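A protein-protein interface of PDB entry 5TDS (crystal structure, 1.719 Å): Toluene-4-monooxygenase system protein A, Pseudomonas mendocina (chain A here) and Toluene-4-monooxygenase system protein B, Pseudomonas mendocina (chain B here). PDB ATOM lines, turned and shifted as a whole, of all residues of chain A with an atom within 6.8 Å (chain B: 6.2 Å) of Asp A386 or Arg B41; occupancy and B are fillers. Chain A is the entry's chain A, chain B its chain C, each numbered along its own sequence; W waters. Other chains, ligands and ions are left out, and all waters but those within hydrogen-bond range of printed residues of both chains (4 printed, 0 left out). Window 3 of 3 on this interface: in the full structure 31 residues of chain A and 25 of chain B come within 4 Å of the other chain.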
ATOM      1  N   TYR A 337       3.260  -8.560   3.472  1.00  0.00           N
ATOM      2  CA  TYR A 337       4.541  -8.387   2.791  1.00  0.00           C
ATOM      3  C   TYR A 337       5.679  -8.412   3.827  1.00  0.00           C
ATOM      4  O   TYR A 337       6.741  -8.988   3.581  1.00  0.00           O
ATOM      5  CB  TYR A 337       4.577  -7.093   1.959  1.00  0.00           C
ATOM      6  CG  TYR A 337       5.684  -7.106   0.922  1.00  0.00           C
ATOM      7  CD1 TYR A 337       5.471  -7.637  -0.354  1.00  0.00           C
ATOM      8  CD2 TYR A 337       6.959  -6.637   1.235  1.00  0.00           C
ATOM      9  CE1 TYR A 337       6.499  -7.675  -1.294  1.00  0.00           C
ATOM     10  CE2 TYR A 337       7.982  -6.666   0.305  1.00  0.00           C
ATOM     11  CZ  TYR A 337       7.748  -7.189  -0.953  1.00  0.00           C
ATOM     12  OH  TYR A 337       8.776  -7.226  -1.869  1.00  0.00           O
ATOM     13  N   CYS A 372      -1.275  -4.398  -6.805  1.00  0.00           N
ATOM     14  CA  CYS A 372      -0.127  -4.862  -6.032  1.00  0.00           C
ATOM     15  C   CYS A 372      -0.132  -6.384  -5.916  1.00  0.00           C
ATOM     16  O   CYS A 372       0.901  -7.037  -6.076  1.00  0.00           O
ATOM     17  CB  CYS A 372      -0.128  -4.234  -4.632  1.00  0.00           C
ATOM     18  SG  CYS A 372      -0.088  -2.420  -4.598  1.00  0.00           S
ATOM     19  N   TRP A 373      -1.298  -6.948  -5.622  1.00  0.00           N
ATOM     20  CA  TRP A 373      -1.402  -8.393  -5.480  1.00  0.00           C
ATOM     21  C   TRP A 373      -1.166  -9.092  -6.821  1.00  0.00           C
ATOM     22  O   TRP A 373      -0.731 -10.237  -6.848  1.00  0.00           O
ATOM     23  CB  TRP A 373      -2.766  -8.790  -4.890  1.00  0.00           C
ATOM     24  CG  TRP A 373      -2.874  -8.522  -3.392  1.00  0.00           C
ATOM     25  CD1 TRP A 373      -3.683  -7.603  -2.772  1.00  0.00           C
ATOM     26  CD2 TRP A 373      -2.138  -9.178  -2.341  1.00  0.00           C
ATOM     27  NE1 TRP A 373      -3.499  -7.655  -1.411  1.00  0.00           N
ATOM     28  CE2 TRP A 373      -2.554  -8.606  -1.120  1.00  0.00           C
ATOM     29  CE3 TRP A 373      -1.170 -10.187  -2.320  1.00  0.00           C
ATOM     30  CZ2 TRP A 373      -2.051  -9.027   0.119  1.00  0.00           C
ATOM     31  CZ3 TRP A 373      -0.657 -10.594  -1.096  1.00  0.00           C
ATOM     32  CH2 TRP A 373      -1.104 -10.016   0.112  1.00  0.00           C
ATOM     33  N   ASP A 374      -1.434  -8.410  -7.932  1.00  0.00           N
ATOM     34  CA  ASP A 374      -1.112  -8.987  -9.240  1.00  0.00           C
ATOM     35  C   ASP A 374       0.391  -9.222  -9.356  1.00  0.00           C
ATOM     36  O   ASP A 374       0.830 -10.269  -9.829  1.00  0.00           O
ATOM     37  CB  ASP A 374      -1.573  -8.088 -10.391  1.00  0.00           C
ATOM     38  CG  ASP A 374      -3.072  -8.097 -10.588  1.00  0.00           C
ATOM     39  OD1 ASP A 374      -3.742  -9.029 -10.099  1.00  0.00           O
ATOM     40  OD2 ASP A 374      -3.579  -7.172 -11.259  1.00  0.00           O
ATOM     41  N   VAL A 375       1.174  -8.233  -8.935  1.00  0.00           N
ATOM     42  CA  VAL A 375       2.632  -8.323  -9.019  1.00  0.00           C
ATOM     43  C   VAL A 375       3.145  -9.415  -8.099  1.00  0.00           C
ATOM     44  O   VAL A 375       3.945 -10.266  -8.496  1.00  0.00           O
ATOM     45  CB  VAL A 375       3.305  -6.994  -8.657  1.00  0.00           C
ATOM     46  CG1 VAL A 375       4.802  -7.144  -8.722  1.00  0.00           C
ATOM     47  CG2 VAL A 375       2.838  -5.892  -9.610  1.00  0.00           C
ATOM     48  N   ILE A 376       2.661  -9.385  -6.868  1.00  0.00           N
ATOM     49  CA  ILE A 376       3.002 -10.393  -5.874  1.00  0.00           C
ATOM     50  C   ILE A 376       2.632 -11.800  -6.343  1.00  0.00           C
ATOM     51  O   ILE A 376       3.424 -12.732  -6.224  1.00  0.00           O
ATOM     52  CB  ILE A 376       2.306 -10.103  -4.530  1.00  0.00           C
ATOM     53  CG1 ILE A 376       2.937  -8.873  -3.865  1.00  0.00           C
ATOM     54  CG2 ILE A 376       2.389 -11.318  -3.612  1.00  0.00           C
ATOM     55  CD1 ILE A 376       2.067  -8.267  -2.779  1.00  0.00           C
ATOM     56  N   THR A 377       1.428 -11.951  -6.886  1.00  0.00           N
ATOM     57  CA  THR A 377       0.964 -13.269  -7.288  1.00  0.00           C
ATOM     58  C   THR A 377       1.807 -13.841  -8.426  1.00  0.00           C
ATOM     59  O   THR A 377       2.158 -15.018  -8.401  1.00  0.00           O
ATOM     60  CB  THR A 377      -0.530 -13.234  -7.702  1.00  0.00           C
ATOM     61  OG1 THR A 377      -1.310 -12.789  -6.586  1.00  0.00           O
ATOM     62  CG2 THR A 377      -1.016 -14.619  -8.135  1.00  0.00           C
ATOM     63  N   ASN A 379       4.868 -13.170  -9.008  1.00  0.00           N
ATOM     64  CA  ASN A 379       6.176 -13.498  -8.448  1.00  0.00           C
ATOM     65  C   ASN A 379       6.134 -14.822  -7.696  1.00  0.00           C
ATOM     66  O   ASN A 379       7.049 -15.630  -7.804  1.00  0.00           O
ATOM     67  CB  ASN A 379       6.686 -12.372  -7.539  1.00  0.00           C
ATOM     68  CG  ASN A 379       7.242 -11.203  -8.334  1.00  0.00           C
ATOM     69  OD1 ASN A 379       7.668 -11.373  -9.477  1.00  0.00           O
ATOM     70  ND2 ASN A 379       7.239 -10.012  -7.735  1.00  0.00           N
ATOM     71  N   ASP A 383       8.105 -18.365  -8.451  1.00  0.00           N
ATOM     72  CA  ASP A 383       8.973 -18.723  -7.333  1.00  0.00           C
ATOM     73  C   ASP A 383      10.026 -17.642  -7.088  1.00  0.00           C
ATOM     74  O   ASP A 383      11.165 -17.936  -6.722  1.00  0.00           O
ATOM     75  CB  ASP A 383       9.645 -20.080  -7.581  1.00  0.00           C
ATOM     76  CG  ASP A 383      10.254 -20.674  -6.318  1.00  0.00           C
ATOM     77  OD1 ASP A 383       9.689 -20.461  -5.221  1.00  0.00           O
ATOM     78  OD2 ASP A 383      11.305 -21.345  -6.422  1.00  0.00           O
ATOM     79  N   ARG A 384       9.644 -16.388  -7.305  1.00  0.00           N
ATOM     80  CA  ARG A 384      10.531 -15.279  -6.988  1.00  0.00           C
ATOM     81  C   ARG A 384      10.316 -14.891  -5.531  1.00  0.00           C
ATOM     82  O   ARG A 384       9.688 -13.873  -5.232  1.00  0.00           O
ATOM     83  CB  ARG A 384      10.287 -14.080  -7.912  1.00  0.00           C
ATOM     84  CG  ARG A 384      10.665 -14.303  -9.378  1.00  0.00           C
ATOM     85  CD  ARG A 384      12.163 -14.549  -9.563  1.00  0.00           C
ATOM     86  NE  ARG A 384      13.008 -13.525  -8.949  1.00  0.00           N
ATOM     87  CZ  ARG A 384      13.458 -12.435  -9.569  1.00  0.00           C
ATOM     88  NH1 ARG A 384      13.131 -12.196 -10.836  1.00  0.00           N
ATOM     89  NH2 ARG A 384      14.237 -11.575  -8.916  1.00  0.00           N
ATOM     90  N   MET A 385      10.824 -15.725  -4.630  1.00  0.00           N
ATOM     91  CA  MET A 385      10.684 -15.479  -3.203  1.00  0.00           C
ATOM     92  C   MET A 385      11.440 -14.229  -2.782  1.00  0.00           C
ATOM     93  O   MET A 385      11.080 -13.594  -1.800  1.00  0.00           O
ATOM     94  CB  MET A 385      11.181 -16.675  -2.392  1.00  0.00           C
ATOM     95  CG  MET A 385      10.307 -17.907  -2.488  1.00  0.00           C
ATOM     96  SD  MET A 385       8.628 -17.628  -1.875  1.00  0.00           S
ATOM     97  CE  MET A 385       7.749 -17.448  -3.440  1.00  0.00           C
ATOM     98  N   ASP A 386      12.495 -13.881  -3.518  1.00  0.00           N
ATOM     99  CA  ASP A 386      13.259 -12.693  -3.175  1.00  0.00           C
ATOM    100  C   ASP A 386      12.398 -11.438  -3.315  1.00  0.00           C
ATOM    101  O   ASP A 386      12.572 -10.467  -2.568  1.00  0.00           O
ATOM    102  CB  ASP A 386      14.529 -12.585  -4.034  1.00  0.00           C
ATOM    103  CG  ASP A 386      14.243 -12.605  -5.538  1.00  0.00           C
ATOM    104  OD1 ASP A 386      13.320 -13.321  -5.984  1.00  0.00           O
ATOM    105  OD2 ASP A 386      14.965 -11.913  -6.284  1.00  0.00           O
ATOM    106  N   LEU A 387      11.453 -11.468  -4.250  1.00  0.00           N
ATOM    107  CA  LEU A 387      10.643 -10.291  -4.545  1.00  0.00           C
ATOM    108  C   LEU A 387       9.405 -10.167  -3.660  1.00  0.00           C
ATOM    109  O   LEU A 387       8.698  -9.161  -3.724  1.00  0.00           O
ATOM    110  CB  LEU A 387      10.229 -10.292  -6.019  1.00  0.00           C
ATOM    111  CG  LEU A 387      11.402 -10.175  -7.001  1.00  0.00           C
ATOM    112  CD1 LEU A 387      10.919 -10.100  -8.436  1.00  0.00           C
ATOM    113  CD2 LEU A 387      12.277  -8.969  -6.669  1.00  0.00           C
ATOM    114  N   VAL A 388       9.147 -11.175  -2.833  1.00  0.00           N
ATOM    115  CA  VAL A 388       8.046 -11.087  -1.873  1.00  0.00           C
ATOM    116  C   VAL A 388       8.604 -11.067  -0.448  1.00  0.00           C
ATOM    117  O   VAL A 388       7.891 -11.312   0.523  1.00  0.00           O
ATOM    118  CB  VAL A 388       7.041 -12.242  -2.042  1.00  0.00           C
ATOM    119  CG1 VAL A 388       6.417 -12.197  -3.430  1.00  0.00           C
ATOM    120  CG2 VAL A 388       7.713 -13.585  -1.803  1.00  0.00           C
ATOM    121  N   SER A 389       9.895 -10.767  -0.344  1.00  0.00           N
ATOM    122  CA  SER A 389      10.573 -10.570   0.936  1.00  0.00           C
ATOM    123  C   SER A 389      11.210  -9.180   0.985  1.00  0.00           C
ATOM    124  O   SER A 389      12.036  -8.857   0.136  1.00  0.00           O
ATOM    125  CB  SER A 389      11.647 -11.636   1.140  1.00  0.00           C
ATOM    126  OG  SER A 389      11.079 -12.930   1.103  1.00  0.00           O
ATOM    127  N   PRO A 390      10.841  -8.360   1.985  1.00  0.00           N
ATOM    128  CA  PRO A 390      11.308  -6.970   2.062  1.00  0.00           C
ATOM    129  C   PRO A 390      12.774  -6.836   2.450  1.00  0.00           C
ATOM    130  O   PRO A 390      13.328  -7.713   3.113  1.00  0.00           O
ATOM    131  CB  PRO A 390      10.420  -6.366   3.156  1.00  0.00           C
ATOM    132  CG  PRO A 390      10.082  -7.525   4.024  1.00  0.00           C
ATOM    133  CD  PRO A 390       9.905  -8.681   3.076  1.00  0.00           C
ATOM    134  N   GLU A 391      13.380  -5.723   2.051  1.00  0.00           N
ATOM    135  CA  GLU A 391      14.782  -5.452   2.356  1.00  0.00           C
ATOM    136  C   GLU A 391      14.950  -4.091   3.008  1.00  0.00           C
ATOM    137  O   GLU A 391      16.069  -3.624   3.214  1.00  0.00           O
ATOM    138  CB  GLU A 391      15.641  -5.508   1.093  1.00  0.00           C
ATOM    139  CG  GLU A 391      15.855  -6.888   0.513  1.00  0.00           C
ATOM    140  CD  GLU A 391      16.881  -6.872  -0.606  1.00  0.00           C
ATOM    141  OE1 GLU A 391      17.737  -5.957  -0.624  1.00  0.00           O
ATOM    142  OE2 GLU A 391      16.841  -7.771  -1.466  1.00  0.00           O
ATOM    143  N   ALA B  35      13.132   2.772  -6.242  1.00  0.00           N
ATOM    144  CA  ALA B  35      12.450   1.839  -7.144  1.00  0.00           C
ATOM    145  C   ALA B  35      12.808   0.381  -6.868  1.00  0.00           C
ATOM    146  O   ALA B  35      11.971  -0.509  -7.033  1.00  0.00           O
ATOM    147  CB  ALA B  35      12.764   2.180  -8.594  1.00  0.00           C
ATOM    148  N   TYR B  36      14.048   0.141  -6.451  1.00  0.00           N
ATOM    149  CA  TYR B  36      14.485  -1.208  -6.085  1.00  0.00           C
ATOM    150  C   TYR B  36      13.528  -1.882  -5.102  1.00  0.00           C
ATOM    151  O   TYR B  36      13.305  -3.091  -5.166  1.00  0.00           O
ATOM    152  CB  TYR B  36      15.883  -1.168  -5.470  1.00  0.00           C
ATOM    153  CG  TYR B  36      16.368  -2.512  -4.982  1.00  0.00           C
ATOM    154  CD1 TYR B  36      17.027  -3.381  -5.837  1.00  0.00           C
ATOM    155  CD2 TYR B  36      16.160  -2.920  -3.670  1.00  0.00           C
ATOM    156  CE1 TYR B  36      17.470  -4.615  -5.407  1.00  0.00           C
ATOM    157  CE2 TYR B  36      16.599  -4.162  -3.228  1.00  0.00           C
ATOM    158  CZ  TYR B  36      17.254  -5.001  -4.107  1.00  0.00           C
ATOM    159  OH  TYR B  36      17.701  -6.231  -3.688  1.00  0.00           O
ATOM    160  N   HIS B  37      12.978  -1.090  -4.188  1.00  0.00           N
ATOM    161  CA  HIS B  37      12.126  -1.617  -3.129  1.00  0.00           C
ATOM    162  C   HIS B  37      10.639  -1.617  -3.482  1.00  0.00           C
ATOM    163  O   HIS B  37       9.804  -1.941  -2.623  1.00  0.00           O
ATOM    164  CB  HIS B  37      12.341  -0.811  -1.846  1.00  0.00           C
ATOM    165  CG  HIS B  37      13.725  -0.922  -1.294  1.00  0.00           C
ATOM    166  ND1 HIS B  37      14.189  -2.066  -0.680  1.00  0.00           N
ATOM    167  CD2 HIS B  37      14.751  -0.036  -1.264  1.00  0.00           C
ATOM    168  CE1 HIS B  37      15.438  -1.879  -0.293  1.00  0.00           C
ATOM    169  NE2 HIS B  37      15.802  -0.654  -0.634  1.00  0.00           N
ATOM    170  N   CYS B  38      10.310  -1.272  -4.730  1.00  0.00           N
ATOM    171  CA  CYS B  38       8.911  -1.127  -5.149  1.00  0.00           C
ATOM    172  C   CYS B  38       8.599  -1.797  -6.484  1.00  0.00           C
ATOM    173  O   CYS B  38       7.669  -2.596  -6.593  1.00  0.00           O
ATOM    174  CB  CYS B  38       8.537   0.358  -5.241  1.00  0.00           C
ATOM    175  SG  CYS B  38       8.932   1.283  -3.751  1.00  0.00           S
ATOM    176  N   VAL B  39       9.370  -1.453  -7.510  1.00  0.00           N
ATOM    177  CA  VAL B  39       9.111  -1.978  -8.845  1.00  0.00           C
ATOM    178  C   VAL B  39       9.343  -3.488  -8.896  1.00  0.00           C
ATOM    179  O   VAL B  39      10.349  -3.989  -8.392  1.00  0.00           O
ATOM    180  CB  VAL B  39       9.980  -1.263  -9.884  1.00  0.00           C
ATOM    181  CG1 VAL B  39       9.772  -1.881 -11.250  1.00  0.00           C
ATOM    182  CG2 VAL B  39       9.636   0.220  -9.895  1.00  0.00           C
ATOM    183  N   ASN B  40       8.381  -4.205  -9.480  1.00  0.00           N
ATOM    184  CA  ASN B  40       8.395  -5.666  -9.539  1.00  0.00           C
ATOM    185  C   ASN B  40       8.254  -6.347  -8.177  1.00  0.00           C
ATOM    186  O   ASN B  40       8.438  -7.562  -8.058  1.00  0.00           O
ATOM    187  CB  ASN B  40       9.660  -6.158 -10.233  1.00  0.00           C
ATOM    188  CG  ASN B  40       9.558  -6.058 -11.736  1.00  0.00           C
ATOM    189  OD1 ASN B  40       8.528  -6.411 -12.324  1.00  0.00           O
ATOM    190  ND2 ASN B  40      10.612  -5.565 -12.371  1.00  0.00           N
ATOM    191  N   ARG B  41       7.917  -5.563  -7.157  1.00  0.00           N
ATOM    192  CA  ARG B  41       7.542  -6.114  -5.857  1.00  0.00           C
ATOM    193  C   ARG B  41       6.055  -5.894  -5.629  1.00  0.00           C
ATOM    194  O   ARG B  41       5.311  -6.843  -5.365  1.00  0.00           O
ATOM    195  CB  ARG B  41       8.357  -5.477  -4.731  1.00  0.00           C
ATOM    196  CG  ARG B  41       9.840  -5.844  -4.792  1.00  0.00           C
ATOM    197  CD  ARG B  41      10.690  -5.128  -3.752  1.00  0.00           C
ATOM    198  NE  ARG B  41      12.079  -5.572  -3.846  1.00  0.00           N
ATOM    199  CZ  ARG B  41      12.569  -6.622  -3.197  1.00  0.00           C
ATOM    200  NH1 ARG B  41      11.790  -7.313  -2.374  1.00  0.00           N
ATOM    201  NH2 ARG B  41      13.839  -6.972  -3.359  1.00  0.00           N
ATOM    202  N   ARG B  42       5.624  -4.643  -5.758  1.00  0.00           N
ATOM    203  CA  ARG B  42       4.213  -4.298  -5.605  1.00  0.00           C
ATOM    204  C   ARG B  42       3.738  -3.339  -6.684  1.00  0.00           C
ATOM    205  O   ARG B  42       2.563  -2.990  -6.729  1.00  0.00           O
ATOM    206  CB  ARG B  42       3.963  -3.690  -4.224  1.00  0.00           C
ATOM    207  CG  ARG B  42       4.261  -4.647  -3.068  1.00  0.00           C
ATOM    208  CD  ARG B  42       4.149  -3.940  -1.730  1.00  0.00           C
ATOM    209  NE  ARG B  42       4.992  -2.753  -1.737  1.00  0.00           N
ATOM    210  CZ  ARG B  42       6.287  -2.759  -1.447  1.00  0.00           C
ATOM    211  NH1 ARG B  42       6.978  -1.634  -1.511  1.00  0.00           N
ATOM    212  NH2 ARG B  42       6.889  -3.890  -1.089  1.00  0.00           N
ATOM    213  N   VAL B  43       4.656  -2.913  -7.548  1.00  0.00           N
ATOM    214  CA  VAL B  43       4.358  -1.961  -8.613  1.00  0.00           C
ATOM    215  C   VAL B  43       4.840  -2.505  -9.951  1.00  0.00           C
ATOM    216  O   VAL B  43       5.968  -2.972 -10.065  1.00  0.00           O
ATOM    217  CB  VAL B  43       5.028  -0.596  -8.335  1.00  0.00           C
ATOM    218  CG1 VAL B  43       4.873   0.338  -9.520  1.00  0.00           C
ATOM    219  CG2 VAL B  43       4.441   0.023  -7.077  1.00  0.00           C
HETATM  220  O   HOH W   1       6.278  -9.291  -5.175  1.00  0.00           O
HETATM  221  O   HOH W   2       0.769  -1.005  -7.966  1.00  0.00           O
HETATM  222  O   HOH W   3      12.350  -4.216  -0.066  1.00  0.00           O
HETATM  223  O   HOH W   4       8.683  -9.706 -11.439  1.00  0.00           O
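Water W1 lies within hydrogen-bond range of O of Arg B41 (2.6 Å), O of Leu A387 (2.8 Å) and ND2 of Asn A379 (2.8 Å).
Water W4 bridges OD1 of Asn A379 (2.8 Å) and OD1 of Asn B40 (3.4 Å).
Water W3 lies within hydrogen-bond range of the backbone NH (N) of Glu A391 and a ring nitrogen (ND1) of His B37.
Water W2 bridges the backbone carbonyl oxygen of Arg B42 (2.9 Å) and the side-chain sulfur of Cys A372 (3.8 Å).
Among the printed residues, merely in contact across the chains: Tyr A337 with Arg B42 (3.3 Å), Val A375 with Arg B41 (3.4 Å), Ile A376 with Arg B41 (3.5 Å), Leu A387 with Asn B40 (3.6 Å), Val A375 with Asn B40 (3.6 Å), Leu A387 with Arg B41 (3.7 Å), Glu A391 with His B37 (3.9 Å), Val A375 with Val B43 (3.9 Å) and Val A375 with Arg B42 (3.96 Å).
The backbone carbonyl oxygen of Leu A387 is in hydrogen-bond range of the side-chain hydroxyl of Tyr A337.
The backbone carbonyl oxygen (O) of Val A375 sits at hydrogen-bond distance from the side-chain amide nitrogen (ND2) of Asn A379, at 3.4 Å.
NH2 of Arg A384 lies within salt-bridge range of OD2 of Asp A386 (2.8 Å).
O of Tyr B36 lies within hydrogen-bond range of NE of Arg B41 (3.1 Å).
O of His B37 lies within hydrogen-bond range of NH1 of Arg B42.
N of Val B43 lies within hydrogen-bond range of O of Cys B38 (3.2 Å).
Of the printed residues of chain B, Cys A372 touches Arg B42.
Asp A386 touches just one residue of chain B: Arg B41 (3.3 Å).
Printed residues of chain A within 4 Å of Asn B40: Val A375, Asn A379 and Leu A387.
Of chain A, only Tyr A337 (3.1 Å), Val A375 (3.4 Å), Ile A376 (3.5 Å), Asp A386 (3.3 Å), Leu A387 (3.7 Å), Ser A389 (3.0 Å) and Glu A391 (3.6 Å) come within 4 Å of Arg B41.
The side-chain hydroxyl (OH) of Tyr A337 sits at hydrogen-bond distance from the guanidinium group (NH1) of Arg B41, 3.1 Å away.
The side-chain sulfur (SG) of Cys A372 sits close to the backbone carbonyl oxygen (O) of Arg B42, at 3.4 Å.
The backbone carbonyl oxygen (O) of Asn B40 lies within hydrogen-bond range of the side-chain amide nitrogen (ND2) of Asn A379, 2.7 Å away.
NH1 of Arg B41 lies within hydrogen-bond range of O of Asp A386, 3.3 Å away.
The guanidinium group (NH1) of Arg B41 sits at hydrogen-bond distance from the backbone carbonyl oxygen (O) of Ser A389, at 3.0 Å.
The side-chain carboxylate of Glu A391 is in hydrogen-bond range of the side-chain hydroxyl of Tyr B36 (2.8 Å).
The side-chain carboxylate (OE2) of Glu A391 lies within salt-bridge range of the guanidinium group (NH2) of Arg B41 (3.6 Å).
Printed residues of chain B that touch a printed residue of chain A: Tyr B36, His B37, Asn B40, Arg B41, Arg B42 and Val B43.
Hydrophobic or aromatic side chains of chain B within 4 Å of the printed part of chain A: Tyr B36 and His B37.
Of the 17 printed residues of chain A, 9 touch a printed residue of chain B.
Along chain A the printed residues that touch a printed residue of chain B span positions 337 to 391.
Among the printed residues, Asp or Glu carboxylates within 4 Å of a Lys or Arg side-chain nitrogen of the other chain: Glu A391 with Arg B41 (3.6 Å).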
